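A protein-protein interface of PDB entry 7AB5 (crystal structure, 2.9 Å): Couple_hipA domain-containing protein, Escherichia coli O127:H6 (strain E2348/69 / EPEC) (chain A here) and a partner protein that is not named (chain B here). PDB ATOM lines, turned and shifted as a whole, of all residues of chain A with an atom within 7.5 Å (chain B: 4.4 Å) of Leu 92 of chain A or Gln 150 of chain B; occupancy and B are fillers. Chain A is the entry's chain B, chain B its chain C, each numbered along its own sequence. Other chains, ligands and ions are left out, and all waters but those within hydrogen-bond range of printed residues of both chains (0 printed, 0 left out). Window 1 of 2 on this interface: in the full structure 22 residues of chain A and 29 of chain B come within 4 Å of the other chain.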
ATOM      1  N   SER A  37      10.967  -4.151 -17.638  1.00  0.00           N
ATOM      2  CA  SER A  37      10.674  -5.294 -18.489  1.00  0.00           C
ATOM      3  C   SER A  37       9.344  -5.872 -18.041  1.00  0.00           C
ATOM      4  O   SER A  37       9.000  -5.804 -16.858  1.00  0.00           O
ATOM      5  CB  SER A  37      11.776  -6.359 -18.403  1.00  0.00           C
ATOM      6  OG  SER A  37      11.354  -7.590 -18.965  1.00  0.00           O
ATOM      7  N   ILE A  38       8.594  -6.433 -18.991  1.00  0.00           N
ATOM      8  CA  ILE A  38       7.341  -7.074 -18.616  1.00  0.00           C
ATOM      9  C   ILE A  38       7.574  -8.354 -17.829  1.00  0.00           C
ATOM     10  O   ILE A  38       6.632  -8.886 -17.232  1.00  0.00           O
ATOM     11  CB  ILE A  38       6.465  -7.354 -19.854  1.00  0.00           C
ATOM     12  CG1 ILE A  38       7.016  -8.526 -20.657  1.00  0.00           C
ATOM     13  CG2 ILE A  38       6.331  -6.111 -20.719  1.00  0.00           C
ATOM     14  CD1 ILE A  38       6.213  -9.779 -20.458  1.00  0.00           C
ATOM     15  N   SER A  39       8.808  -8.864 -17.818  1.00  0.00           N
ATOM     16  CA  SER A  39       9.154  -9.986 -16.959  1.00  0.00           C
ATOM     17  C   SER A  39       9.338  -9.566 -15.507  1.00  0.00           C
ATOM     18  O   SER A  39       9.316 -10.426 -14.621  1.00  0.00           O
ATOM     19  CB  SER A  39      10.433 -10.664 -17.458  1.00  0.00           C
ATOM     20  OG  SER A  39      11.461  -9.715 -17.680  1.00  0.00           O
ATOM     21  N   PRO A  54      16.245 -14.018 -16.596  1.00  0.00           N
ATOM     22  CA  PRO A  54      16.405 -14.086 -18.057  1.00  0.00           C
ATOM     23  C   PRO A  54      16.447 -12.725 -18.724  1.00  0.00           C
ATOM     24  O   PRO A  54      17.086 -12.585 -19.775  1.00  0.00           O
ATOM     25  CB  PRO A  54      15.184 -14.898 -18.506  1.00  0.00           C
ATOM     26  CG  PRO A  54      14.760 -15.657 -17.294  1.00  0.00           C
ATOM     27  CD  PRO A  54      15.061 -14.761 -16.134  1.00  0.00           C
ATOM     28  N   TYR A  55      15.793 -11.716 -18.148  1.00  0.00           N
ATOM     29  CA  TYR A  55      15.918 -10.370 -18.692  1.00  0.00           C
ATOM     30  C   TYR A  55      17.368  -9.907 -18.660  1.00  0.00           C
ATOM     31  O   TYR A  55      17.926  -9.505 -19.688  1.00  0.00           O
ATOM     32  CB  TYR A  55      15.032  -9.388 -17.927  1.00  0.00           C
ATOM     33  CG  TYR A  55      15.217  -7.964 -18.401  1.00  0.00           C
ATOM     34  CD1 TYR A  55      14.781  -7.577 -19.661  1.00  0.00           C
ATOM     35  CD2 TYR A  55      15.844  -7.013 -17.604  1.00  0.00           C
ATOM     36  CE1 TYR A  55      14.951  -6.282 -20.113  1.00  0.00           C
ATOM     37  CE2 TYR A  55      16.018  -5.712 -18.046  1.00  0.00           C
ATOM     38  CZ  TYR A  55      15.572  -5.353 -19.303  1.00  0.00           C
ATOM     39  OH  TYR A  55      15.742  -4.063 -19.753  1.00  0.00           O
ATOM     40  N   SER A  58      19.856 -11.482 -20.993  1.00  0.00           N
ATOM     41  CA  SER A  58      19.633 -11.162 -22.396  1.00  0.00           C
ATOM     42  C   SER A  58      20.130  -9.773 -22.787  1.00  0.00           C
ATOM     43  O   SER A  58      20.259  -9.498 -23.985  1.00  0.00           O
ATOM     44  CB  SER A  58      18.145 -11.288 -22.733  1.00  0.00           C
ATOM     45  OG  SER A  58      17.473 -10.054 -22.547  1.00  0.00           O
ATOM     46  N   LEU A  59      20.409  -8.890 -21.823  1.00  0.00           N
ATOM     47  CA  LEU A  59      20.957  -7.590 -22.194  1.00  0.00           C
ATOM     48  C   LEU A  59      22.431  -7.661 -22.562  1.00  0.00           C
ATOM     49  O   LEU A  59      22.941  -6.723 -23.184  1.00  0.00           O
ATOM     50  CB  LEU A  59      20.778  -6.554 -21.081  1.00  0.00           C
ATOM     51  CG  LEU A  59      19.367  -6.172 -20.632  1.00  0.00           C
ATOM     52  CD1 LEU A  59      19.095  -6.643 -19.223  1.00  0.00           C
ATOM     53  CD2 LEU A  59      19.160  -4.675 -20.749  1.00  0.00           C
ATOM     54  N   PRO A  61      25.601  -8.534 -24.757  1.00  0.00           N
ATOM     55  CA  PRO A  61      25.765  -8.771 -26.192  1.00  0.00           C
ATOM     56  C   PRO A  61      26.424 -10.115 -26.460  1.00  0.00           C
ATOM     57  O   PRO A  61      27.182 -10.641 -25.645  1.00  0.00           O
ATOM     58  CB  PRO A  61      26.676  -7.620 -26.625  1.00  0.00           C
ATOM     59  CG  PRO A  61      27.564  -7.427 -25.431  1.00  0.00           C
ATOM     60  CD  PRO A  61      26.691  -7.700 -24.214  1.00  0.00           C
ATOM     61  N   ASN A  87      29.628  -3.685 -19.801  1.00  0.00           N
ATOM     62  CA  ASN A  87      28.907  -3.164 -20.953  1.00  0.00           C
ATOM     63  C   ASN A  87      27.730  -2.277 -20.568  1.00  0.00           C
ATOM     64  O   ASN A  87      27.015  -1.808 -21.458  1.00  0.00           O
ATOM     65  CB  ASN A  87      28.408  -4.318 -21.831  1.00  0.00           C
ATOM     66  CG  ASN A  87      29.297  -5.543 -21.748  1.00  0.00           C
ATOM     67  OD1 ASN A  87      30.424  -5.542 -22.243  1.00  0.00           O
ATOM     68  ND2 ASN A  87      28.790  -6.601 -21.126  1.00  0.00           N
ATOM     69  N   GLY A  88      27.530  -2.022 -19.275  1.00  0.00           N
ATOM     70  CA  GLY A  88      26.350  -1.345 -18.764  1.00  0.00           C
ATOM     71  C   GLY A  88      25.921  -0.069 -19.458  1.00  0.00           C
ATOM     72  O   GLY A  88      24.722   0.197 -19.575  1.00  0.00           O
ATOM     73  N   LYS A  89      26.878   0.732 -19.921  1.00  0.00           N
ATOM     74  CA  LYS A  89      26.556   2.003 -20.556  1.00  0.00           C
ATOM     75  C   LYS A  89      26.262   1.875 -22.045  1.00  0.00           C
ATOM     76  O   LYS A  89      25.796   2.846 -22.652  1.00  0.00           O
ATOM     77  CB  LYS A  89      27.694   3.007 -20.337  1.00  0.00           C
ATOM     78  CG  LYS A  89      28.958   2.405 -19.743  1.00  0.00           C
ATOM     79  CD  LYS A  89      29.297   3.030 -18.392  1.00  0.00           C
ATOM     80  CE  LYS A  89      28.959   4.516 -18.342  1.00  0.00           C
ATOM     81  NZ  LYS A  89      30.160   5.350 -18.061  1.00  0.00           N
ATOM     82  N   ASN A  90      26.509   0.713 -22.645  1.00  0.00           N
ATOM     83  CA  ASN A  90      26.253   0.475 -24.060  1.00  0.00           C
ATOM     84  C   ASN A  90      25.136  -0.544 -24.260  1.00  0.00           C
ATOM     85  O   ASN A  90      25.235  -1.451 -25.089  1.00  0.00           O
ATOM     86  CB  ASN A  90      27.525   0.022 -24.771  1.00  0.00           C
ATOM     87  CG  ASN A  90      27.780   0.793 -26.049  1.00  0.00           C
ATOM     88  OD1 ASN A  90      27.787   2.022 -26.055  1.00  0.00           O
ATOM     89  ND2 ASN A  90      28.004   0.071 -27.137  1.00  0.00           N
ATOM     90  N   LEU A  91      24.060  -0.399 -23.497  1.00  0.00           N
ATOM     91  CA  LEU A  91      22.926  -1.307 -23.557  1.00  0.00           C
ATOM     92  C   LEU A  91      21.844  -0.748 -24.476  1.00  0.00           C
ATOM     93  O   LEU A  91      21.698   0.467 -24.630  1.00  0.00           O
ATOM     94  CB  LEU A  91      22.354  -1.546 -22.156  1.00  0.00           C
ATOM     95  CG  LEU A  91      23.206  -2.313 -21.138  1.00  0.00           C
ATOM     96  CD1 LEU A  91      22.327  -3.121 -20.200  1.00  0.00           C
ATOM     97  CD2 LEU A  91      24.208  -3.227 -21.826  1.00  0.00           C
ATOM     98  N   LEU A  92      21.089  -1.656 -25.088  1.00  0.00           N
ATOM     99  CA  LEU A  92      19.981  -1.254 -25.942  1.00  0.00           C
ATOM    100  C   LEU A  92      18.848  -0.667 -25.109  1.00  0.00           C
ATOM    101  O   LEU A  92      18.513  -1.177 -24.036  1.00  0.00           O
ATOM    102  CB  LEU A  92      19.468  -2.446 -26.748  1.00  0.00           C
ATOM    103  CG  LEU A  92      20.145  -2.765 -28.082  1.00  0.00           C
ATOM    104  CD1 LEU A  92      20.188  -4.269 -28.322  1.00  0.00           C
ATOM    105  CD2 LEU A  92      19.430  -2.055 -29.221  1.00  0.00           C
ATOM    106  N   GLY A  93      18.255   0.412 -25.612  1.00  0.00           N
ATOM    107  CA  GLY A  93      17.133   1.030 -24.938  1.00  0.00           C
ATOM    108  C   GLY A  93      17.525   2.144 -23.991  1.00  0.00           C
ATOM    109  O   GLY A  93      18.463   2.900 -24.261  1.00  0.00           O
ATOM    110  N   ALA A  94      16.808   2.252 -22.873  1.00  0.00           N
ATOM    111  CA  ALA A  94      17.007   3.324 -21.907  1.00  0.00           C
ATOM    112  C   ALA A  94      17.451   2.786 -20.551  1.00  0.00           C
ATOM    113  O   ALA A  94      17.139   3.371 -19.512  1.00  0.00           O
ATOM    114  CB  ALA A  94      15.733   4.152 -21.757  1.00  0.00           C
ATOM    115  N   ILE A  95      18.190   1.680 -20.544  1.00  0.00           N
ATOM    116  CA  ILE A  95      18.588   1.008 -19.314  1.00  0.00           C
ATOM    117  C   ILE A  95      20.105   1.053 -19.189  1.00  0.00           C
ATOM    118  O   ILE A  95      20.827   0.908 -20.182  1.00  0.00           O
ATOM    119  CB  ILE A  95      18.064  -0.443 -19.274  1.00  0.00           C
ATOM    120  CG1 ILE A  95      18.430  -1.113 -17.947  1.00  0.00           C
ATOM    121  CG2 ILE A  95      18.576  -1.232 -20.476  1.00  0.00           C
ATOM    122  CD1 ILE A  95      18.156  -2.597 -17.910  1.00  0.00           C
ATOM    123  N   GLN A  96      20.586   1.276 -17.965  1.00  0.00           N
ATOM    124  CA  GLN A  96      22.010   1.323 -17.669  1.00  0.00           C
ATOM    125  C   GLN A  96      22.305   0.496 -16.428  1.00  0.00           C
ATOM    126  O   GLN A  96      21.521   0.487 -15.474  1.00  0.00           O
ATOM    127  CB  GLN A  96      22.499   2.761 -17.451  1.00  0.00           C
ATOM    128  CG  GLN A  96      21.779   3.812 -18.277  1.00  0.00           C
ATOM    129  CD  GLN A  96      22.548   5.116 -18.345  1.00  0.00           C
ATOM    130  OE1 GLN A  96      23.767   5.139 -18.179  1.00  0.00           O
ATOM    131  NE2 GLN A  96      21.836   6.210 -18.587  1.00  0.00           N
ATOM    132  N   ARG B 136      19.129   3.115 -35.768  1.00  0.00           N
ATOM    133  CA  ARG B 136      18.613   2.445 -34.583  1.00  0.00           C
ATOM    134  C   ARG B 136      17.172   2.863 -34.322  1.00  0.00           C
ATOM    135  O   ARG B 136      16.821   4.041 -34.422  1.00  0.00           O
ATOM    136  CB  ARG B 136      19.488   2.764 -33.372  1.00  0.00           C
ATOM    137  CG  ARG B 136      20.865   2.124 -33.425  1.00  0.00           C
ATOM    138  CD  ARG B 136      21.756   2.618 -32.298  1.00  0.00           C
ATOM    139  NE  ARG B 136      21.321   2.120 -30.998  1.00  0.00           N
ATOM    140  CZ  ARG B 136      22.119   1.966 -29.951  1.00  0.00           C
ATOM    141  NH1 ARG B 136      23.409   2.251 -30.016  1.00  0.00           N
ATOM    142  NH2 ARG B 136      21.611   1.510 -28.810  1.00  0.00           N
ATOM    143  N   TYR B 137      16.334   1.883 -33.991  1.00  0.00           N
ATOM    144  CA  TYR B 137      14.927   2.138 -33.715  1.00  0.00           C
ATOM    145  C   TYR B 137      14.667   2.557 -32.275  1.00  0.00           C
ATOM    146  O   TYR B 137      13.576   3.058 -31.982  1.00  0.00           O
ATOM    147  CB  TYR B 137      14.090   0.899 -34.058  1.00  0.00           C
ATOM    148  CG  TYR B 137      14.343  -0.294 -33.164  1.00  0.00           C
ATOM    149  CD1 TYR B 137      13.630  -0.472 -31.983  1.00  0.00           C
ATOM    150  CD2 TYR B 137      15.295  -1.246 -33.502  1.00  0.00           C
ATOM    151  CE1 TYR B 137      13.860  -1.560 -31.166  1.00  0.00           C
ATOM    152  CE2 TYR B 137      15.532  -2.338 -32.692  1.00  0.00           C
ATOM    153  CZ  TYR B 137      14.812  -2.491 -31.526  1.00  0.00           C
ATOM    154  OH  TYR B 137      15.045  -3.578 -30.716  1.00  0.00           O
ATOM    155  N   ASP B 138      15.627   2.364 -31.372  1.00  0.00           N
ATOM    156  CA  ASP B 138      15.510   2.859 -29.999  1.00  0.00           C
ATOM    157  C   ASP B 138      15.986   4.300 -29.878  1.00  0.00           C
ATOM    158  O   ASP B 138      16.650   4.678 -28.909  1.00  0.00           O
ATOM    159  CB  ASP B 138      16.265   1.946 -29.039  1.00  0.00           C
ATOM    160  CG  ASP B 138      17.680   1.649 -29.498  1.00  0.00           C
ATOM    161  OD1 ASP B 138      17.854   1.189 -30.646  1.00  0.00           O
ATOM    162  OD2 ASP B 138      18.618   1.861 -28.701  1.00  0.00           O
ATOM    163  N   GLN B 148      13.293  -0.301 -24.906  1.00  0.00           N
ATOM    164  CA  GLN B 148      12.898  -1.472 -25.670  1.00  0.00           C
ATOM    165  C   GLN B 148      13.401  -2.711 -24.941  1.00  0.00           C
ATOM    166  O   GLN B 148      14.090  -2.618 -23.921  1.00  0.00           O
ATOM    167  CB  GLN B 148      13.440  -1.412 -27.100  1.00  0.00           C
ATOM    168  CG  GLN B 148      14.947  -1.529 -27.171  1.00  0.00           C
ATOM    169  CD  GLN B 148      15.393  -2.921 -27.559  1.00  0.00           C
ATOM    170  OE1 GLN B 148      14.804  -3.553 -28.436  1.00  0.00           O
ATOM    171  NE2 GLN B 148      16.420  -3.419 -26.886  1.00  0.00           N
ATOM    172  N   GLU B 149      13.067  -3.880 -25.486  1.00  0.00           N
ATOM    173  CA  GLU B 149      13.430  -5.138 -24.850  1.00  0.00           C
ATOM    174  C   GLU B 149      13.164  -6.276 -25.823  1.00  0.00           C
ATOM    175  O   GLU B 149      12.161  -6.261 -26.540  1.00  0.00           O
ATOM    176  CB  GLU B 149      12.641  -5.327 -23.546  1.00  0.00           C
ATOM    177  CG  GLU B 149      12.523  -6.749 -23.037  1.00  0.00           C
ATOM    178  CD  GLU B 149      11.280  -6.941 -22.192  1.00  0.00           C
ATOM    179  OE1 GLU B 149      10.481  -5.986 -22.082  1.00  0.00           O
ATOM    180  OE2 GLU B 149      11.118  -8.032 -21.609  1.00  0.00           O
ATOM    181  N   GLN B 150      14.075  -7.245 -25.854  1.00  0.00           N
ATOM    182  CA  GLN B 150      13.975  -8.369 -26.773  1.00  0.00           C
ATOM    183  C   GLN B 150      13.084  -9.461 -26.191  1.00  0.00           C
ATOM    184  O   GLN B 150      12.893  -9.565 -24.977  1.00  0.00           O
ATOM    185  CB  GLN B 150      15.363  -8.923 -27.097  1.00  0.00           C
ATOM    186  CG  GLN B 150      15.913  -8.419 -28.421  1.00  0.00           C
ATOM    187  CD  GLN B 150      16.498  -7.024 -28.312  1.00  0.00           C
ATOM    188  OE1 GLN B 150      17.266  -6.731 -27.394  1.00  0.00           O
ATOM    189  NE2 GLN B 150      16.129  -6.152 -29.243  1.00  0.00           N
ATOM    190  N   LEU B 151      12.542 -10.292 -27.086  1.00  0.00           N
ATOM    191  CA  LEU B 151      11.456 -11.187 -26.699  1.00  0.00           C
ATOM    192  C   LEU B 151      11.934 -12.307 -25.783  1.00  0.00           C
ATOM    193  O   LEU B 151      11.202 -12.718 -24.877  1.00  0.00           O
ATOM    194  CB  LEU B 151      10.775 -11.762 -27.940  1.00  0.00           C
ATOM    195  CG  LEU B 151       9.404 -11.158 -28.244  1.00  0.00           C
ATOM    196  CD1 LEU B 151       8.375 -11.658 -27.246  1.00  0.00           C
ATOM    197  CD2 LEU B 151       9.477  -9.637 -28.228  1.00  0.00           C
ATOM    198  N   ASP B 152      13.150 -12.819 -25.999  1.00  0.00           N
ATOM    199  CA  ASP B 152      13.629 -13.927 -25.175  1.00  0.00           C
ATOM    200  C   ASP B 152      13.636 -13.552 -23.697  1.00  0.00           C
ATOM    201  O   ASP B 152      13.228 -14.351 -22.846  1.00  0.00           O
ATOM    202  CB  ASP B 152      15.020 -14.370 -25.631  1.00  0.00           C
ATOM    203  CG  ASP B 152      16.102 -13.371 -25.274  1.00  0.00           C
ATOM    204  OD1 ASP B 152      15.856 -12.153 -25.408  1.00  0.00           O
ATOM    205  OD2 ASP B 152      17.195 -13.804 -24.849  1.00  0.00           O
ATOM    206  N   GLY B 153      14.070 -12.332 -23.376  1.00  0.00           N
ATOM    207  CA  GLY B 153      14.062 -11.899 -21.988  1.00  0.00           C
ATOM    208  C   GLY B 153      12.661 -11.633 -21.472  1.00  0.00           C
ATOM    209  O   GLY B 153      12.361 -11.895 -20.304  1.00  0.00           O
ATOM    210  N   ALA B 154      11.786 -11.111 -22.334  1.00  0.00           N
ATOM    211  CA  ALA B 154      10.407 -10.847 -21.932  1.00  0.00           C
ATOM    212  C   ALA B 154       9.695 -12.133 -21.536  1.00  0.00           C
ATOM    213  O   ALA B 154       9.082 -12.214 -20.465  1.00  0.00           O
ATOM    214  CB  ALA B 154       9.658 -10.141 -23.062  1.00  0.00           C
ATOM    215  N   LEU B 212      14.272 -15.486 -31.019  1.00  0.00           N
ATOM    216  CA  LEU B 212      13.536 -14.669 -30.063  1.00  0.00           C
ATOM    217  C   LEU B 212      14.161 -13.298 -29.852  1.00  0.00           C
ATOM    218  O   LEU B 212      13.484 -12.394 -29.351  1.00  0.00           O
ATOM    219  CB  LEU B 212      13.430 -15.410 -28.732  1.00  0.00           C
ATOM    220  CG  LEU B 212      12.485 -16.611 -28.770  1.00  0.00           C
ATOM    221  CD1 LEU B 212      12.535 -17.386 -27.467  1.00  0.00           C
ATOM    222  CD2 LEU B 212      11.077 -16.149 -29.065  1.00  0.00           C
ATOM    223  N   ARG B 213      15.426 -13.116 -30.216  1.00  0.00           N
ATOM    224  CA  ARG B 213      16.089 -11.832 -30.048  1.00  0.00           C
ATOM    225  C   ARG B 213      16.010 -10.973 -31.300  1.00  0.00           C
ATOM    226  O   ARG B 213      16.474  -9.828 -31.283  1.00  0.00           O
ATOM    227  CB  ARG B 213      17.546 -12.045 -29.635  1.00  0.00           C
ATOM    228  CG  ARG B 213      17.695 -13.011 -28.472  1.00  0.00           C
ATOM    229  CD  ARG B 213      18.729 -12.528 -27.478  1.00  0.00           C
ATOM    230  NE  ARG B 213      19.946 -12.094 -28.149  1.00  0.00           N
ATOM    231  CZ  ARG B 213      20.670 -11.048 -27.775  1.00  0.00           C
ATOM    232  NH1 ARG B 213      20.363 -10.345 -26.698  1.00  0.00           N
ATOM    233  NH2 ARG B 213      21.728 -10.700 -28.501  1.00  0.00           N
ATOM    234  N   PHE B 215      12.983 -10.415 -32.338  1.00  0.00           N
ATOM    235  CA  PHE B 215      11.719  -9.781 -31.997  1.00  0.00           C
ATOM    236  C   PHE B 215      11.967  -8.802 -30.856  1.00  0.00           C
ATOM    237  O   PHE B 215      12.768  -9.080 -29.958  1.00  0.00           O
ATOM    238  CB  PHE B 215      10.678 -10.812 -31.553  1.00  0.00           C
ATOM    239  CG  PHE B 215      10.120 -11.652 -32.665  1.00  0.00           C
ATOM    240  CD1 PHE B 215      10.777 -12.799 -33.077  1.00  0.00           C
ATOM    241  CD2 PHE B 215       8.913 -11.324 -33.260  1.00  0.00           C
ATOM    242  CE1 PHE B 215      10.257 -13.587 -34.084  1.00  0.00           C
ATOM    243  CE2 PHE B 215       8.387 -12.109 -34.268  1.00  0.00           C
ATOM    244  CZ  PHE B 215       9.058 -13.244 -34.677  1.00  0.00           C
ATOM    245  N   GLY B 216      11.272  -7.667 -30.875  1.00  0.00           N
ATOM    246  CA  GLY B 216      11.466  -6.661 -29.851  1.00  0.00           C
ATOM    247  C   GLY B 216      10.169  -5.967 -29.486  1.00  0.00           C
ATOM    248  O   GLY B 216       9.211  -5.933 -30.260  1.00  0.00           O
ATOM    249  N   TYR B 231      13.917  -6.109 -38.086  1.00  0.00           N
ATOM    250  CA  TYR B 231      15.363  -5.991 -38.177  1.00  0.00           C
ATOM    251  C   TYR B 231      15.955  -7.389 -38.273  1.00  0.00           C
ATOM    252  O   TYR B 231      15.324  -8.379 -37.893  1.00  0.00           O
ATOM    253  CB  TYR B 231      15.950  -5.218 -36.984  1.00  0.00           C
ATOM    254  CG  TYR B 231      15.649  -5.816 -35.624  1.00  0.00           C
ATOM    255  CD1 TYR B 231      14.499  -5.464 -34.928  1.00  0.00           C
ATOM    256  CD2 TYR B 231      16.525  -6.714 -35.028  1.00  0.00           C
ATOM    257  CE1 TYR B 231      14.225  -6.003 -33.684  1.00  0.00           C
ATOM    258  CE2 TYR B 231      16.259  -7.257 -33.785  1.00  0.00           C
ATOM    259  CZ  TYR B 231      15.108  -6.899 -33.117  1.00  0.00           C
ATOM    260  OH  TYR B 231      14.840  -7.437 -31.879  1.00  0.00           O
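The side-chain hydroxyl of Ser 37 of chain A sits at hydrogen-bond distance from the side-chain carboxylate of Glu 149 of chain B. The guanidinium group (NH1) of Arg 213 of chain B sits at hydrogen-bond distance from the backbone carbonyl oxygen (O) of Ser 58 of chain A, at 2.8 Å. The backbone NH of Gly 93 of chain A lies within hydrogen-bond range of the side-chain carboxylate of Asp 138 of chain B, 3.4 Å away.
OG of Ser 58 of chain A is in hydrogen-bond range of O of Tyr 55 of chain A (2.9 Å). The guanidinium group (NH2) of Arg 136 of chain B is in salt-bridge range of the side-chain carboxylate (OD2) of Asp 138 of chain B. The side-chain amide oxygen (OE1) of Gln 148 of chain B is in hydrogen-bond range of the side-chain amide nitrogen (NE2) of Gln 150 of chain B (3.0 Å). The backbone NH of Ala 154 of chain B lies close to the side-chain carboxylate of Glu 149 of chain B, at 3.2 Å. NE2 of Gln 150 of chain B is in hydrogen-bond range of OH of Tyr 231 of chain B (3.2 Å). O of Leu 212 of chain B lies within hydrogen-bond range of N of Asp 152 of chain B (3.4 Å).
Glu 149 of chain B touches Ile 38 of chain A. Ile 38 of chain A touches Ala 154 of chain B. O of Gly 153 of chain B touches OG of Ser 39 of chain A (3.5 Å). Ser 39 of chain A touches Ala 154 of chain B (CB to O, 3.6 Å). Pro 54 of chain A touches Gly 153 of chain B. Ser 58 of chain A touches Asp 152 of chain B. OG of Ser 58 of chain A touches CA of Gly 153 of chain B (3.9 Å). Leu 92 of chain A touches Asp 138 of chain B (CD2 to OD1, 3.9 Å). Gln 148 of chain B touches Leu 92 of chain A. OE1 of Gln 150 of chain B touches CD1 of Leu 92 of chain A, 3.9 Å away.
Gln 150 of chain B touches just one residue of chain A: Leu 92. Printed residues of chain B within 4 Å of Gly 93 of chain A: Asp 138. Of the printed residues of chain A, Glu 149 of chain B touches Ser 37, Ile 38 and Tyr 55. Leu 212 of chain B touches none of the printed residues of chain A. The nearest residue of chain B that does not touch Leu 92 of chain A is Arg 136 of chain B (4.2 Å).
Of the 15 printed residues of chain B, 8 touch a printed residue of chain A. Printed residues of chain B that touch a printed residue of chain A: Asp 138, Gln 148, Glu 149, Gln 150, Asp 152, Gly 153, Ala 154 and Arg 213. Hydrophobic or aromatic side chains of chain B within 4 Å of the printed part of chain A: Ala 154. Of the 18 printed residues of chain A, 8 touch a printed residue of chain B.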
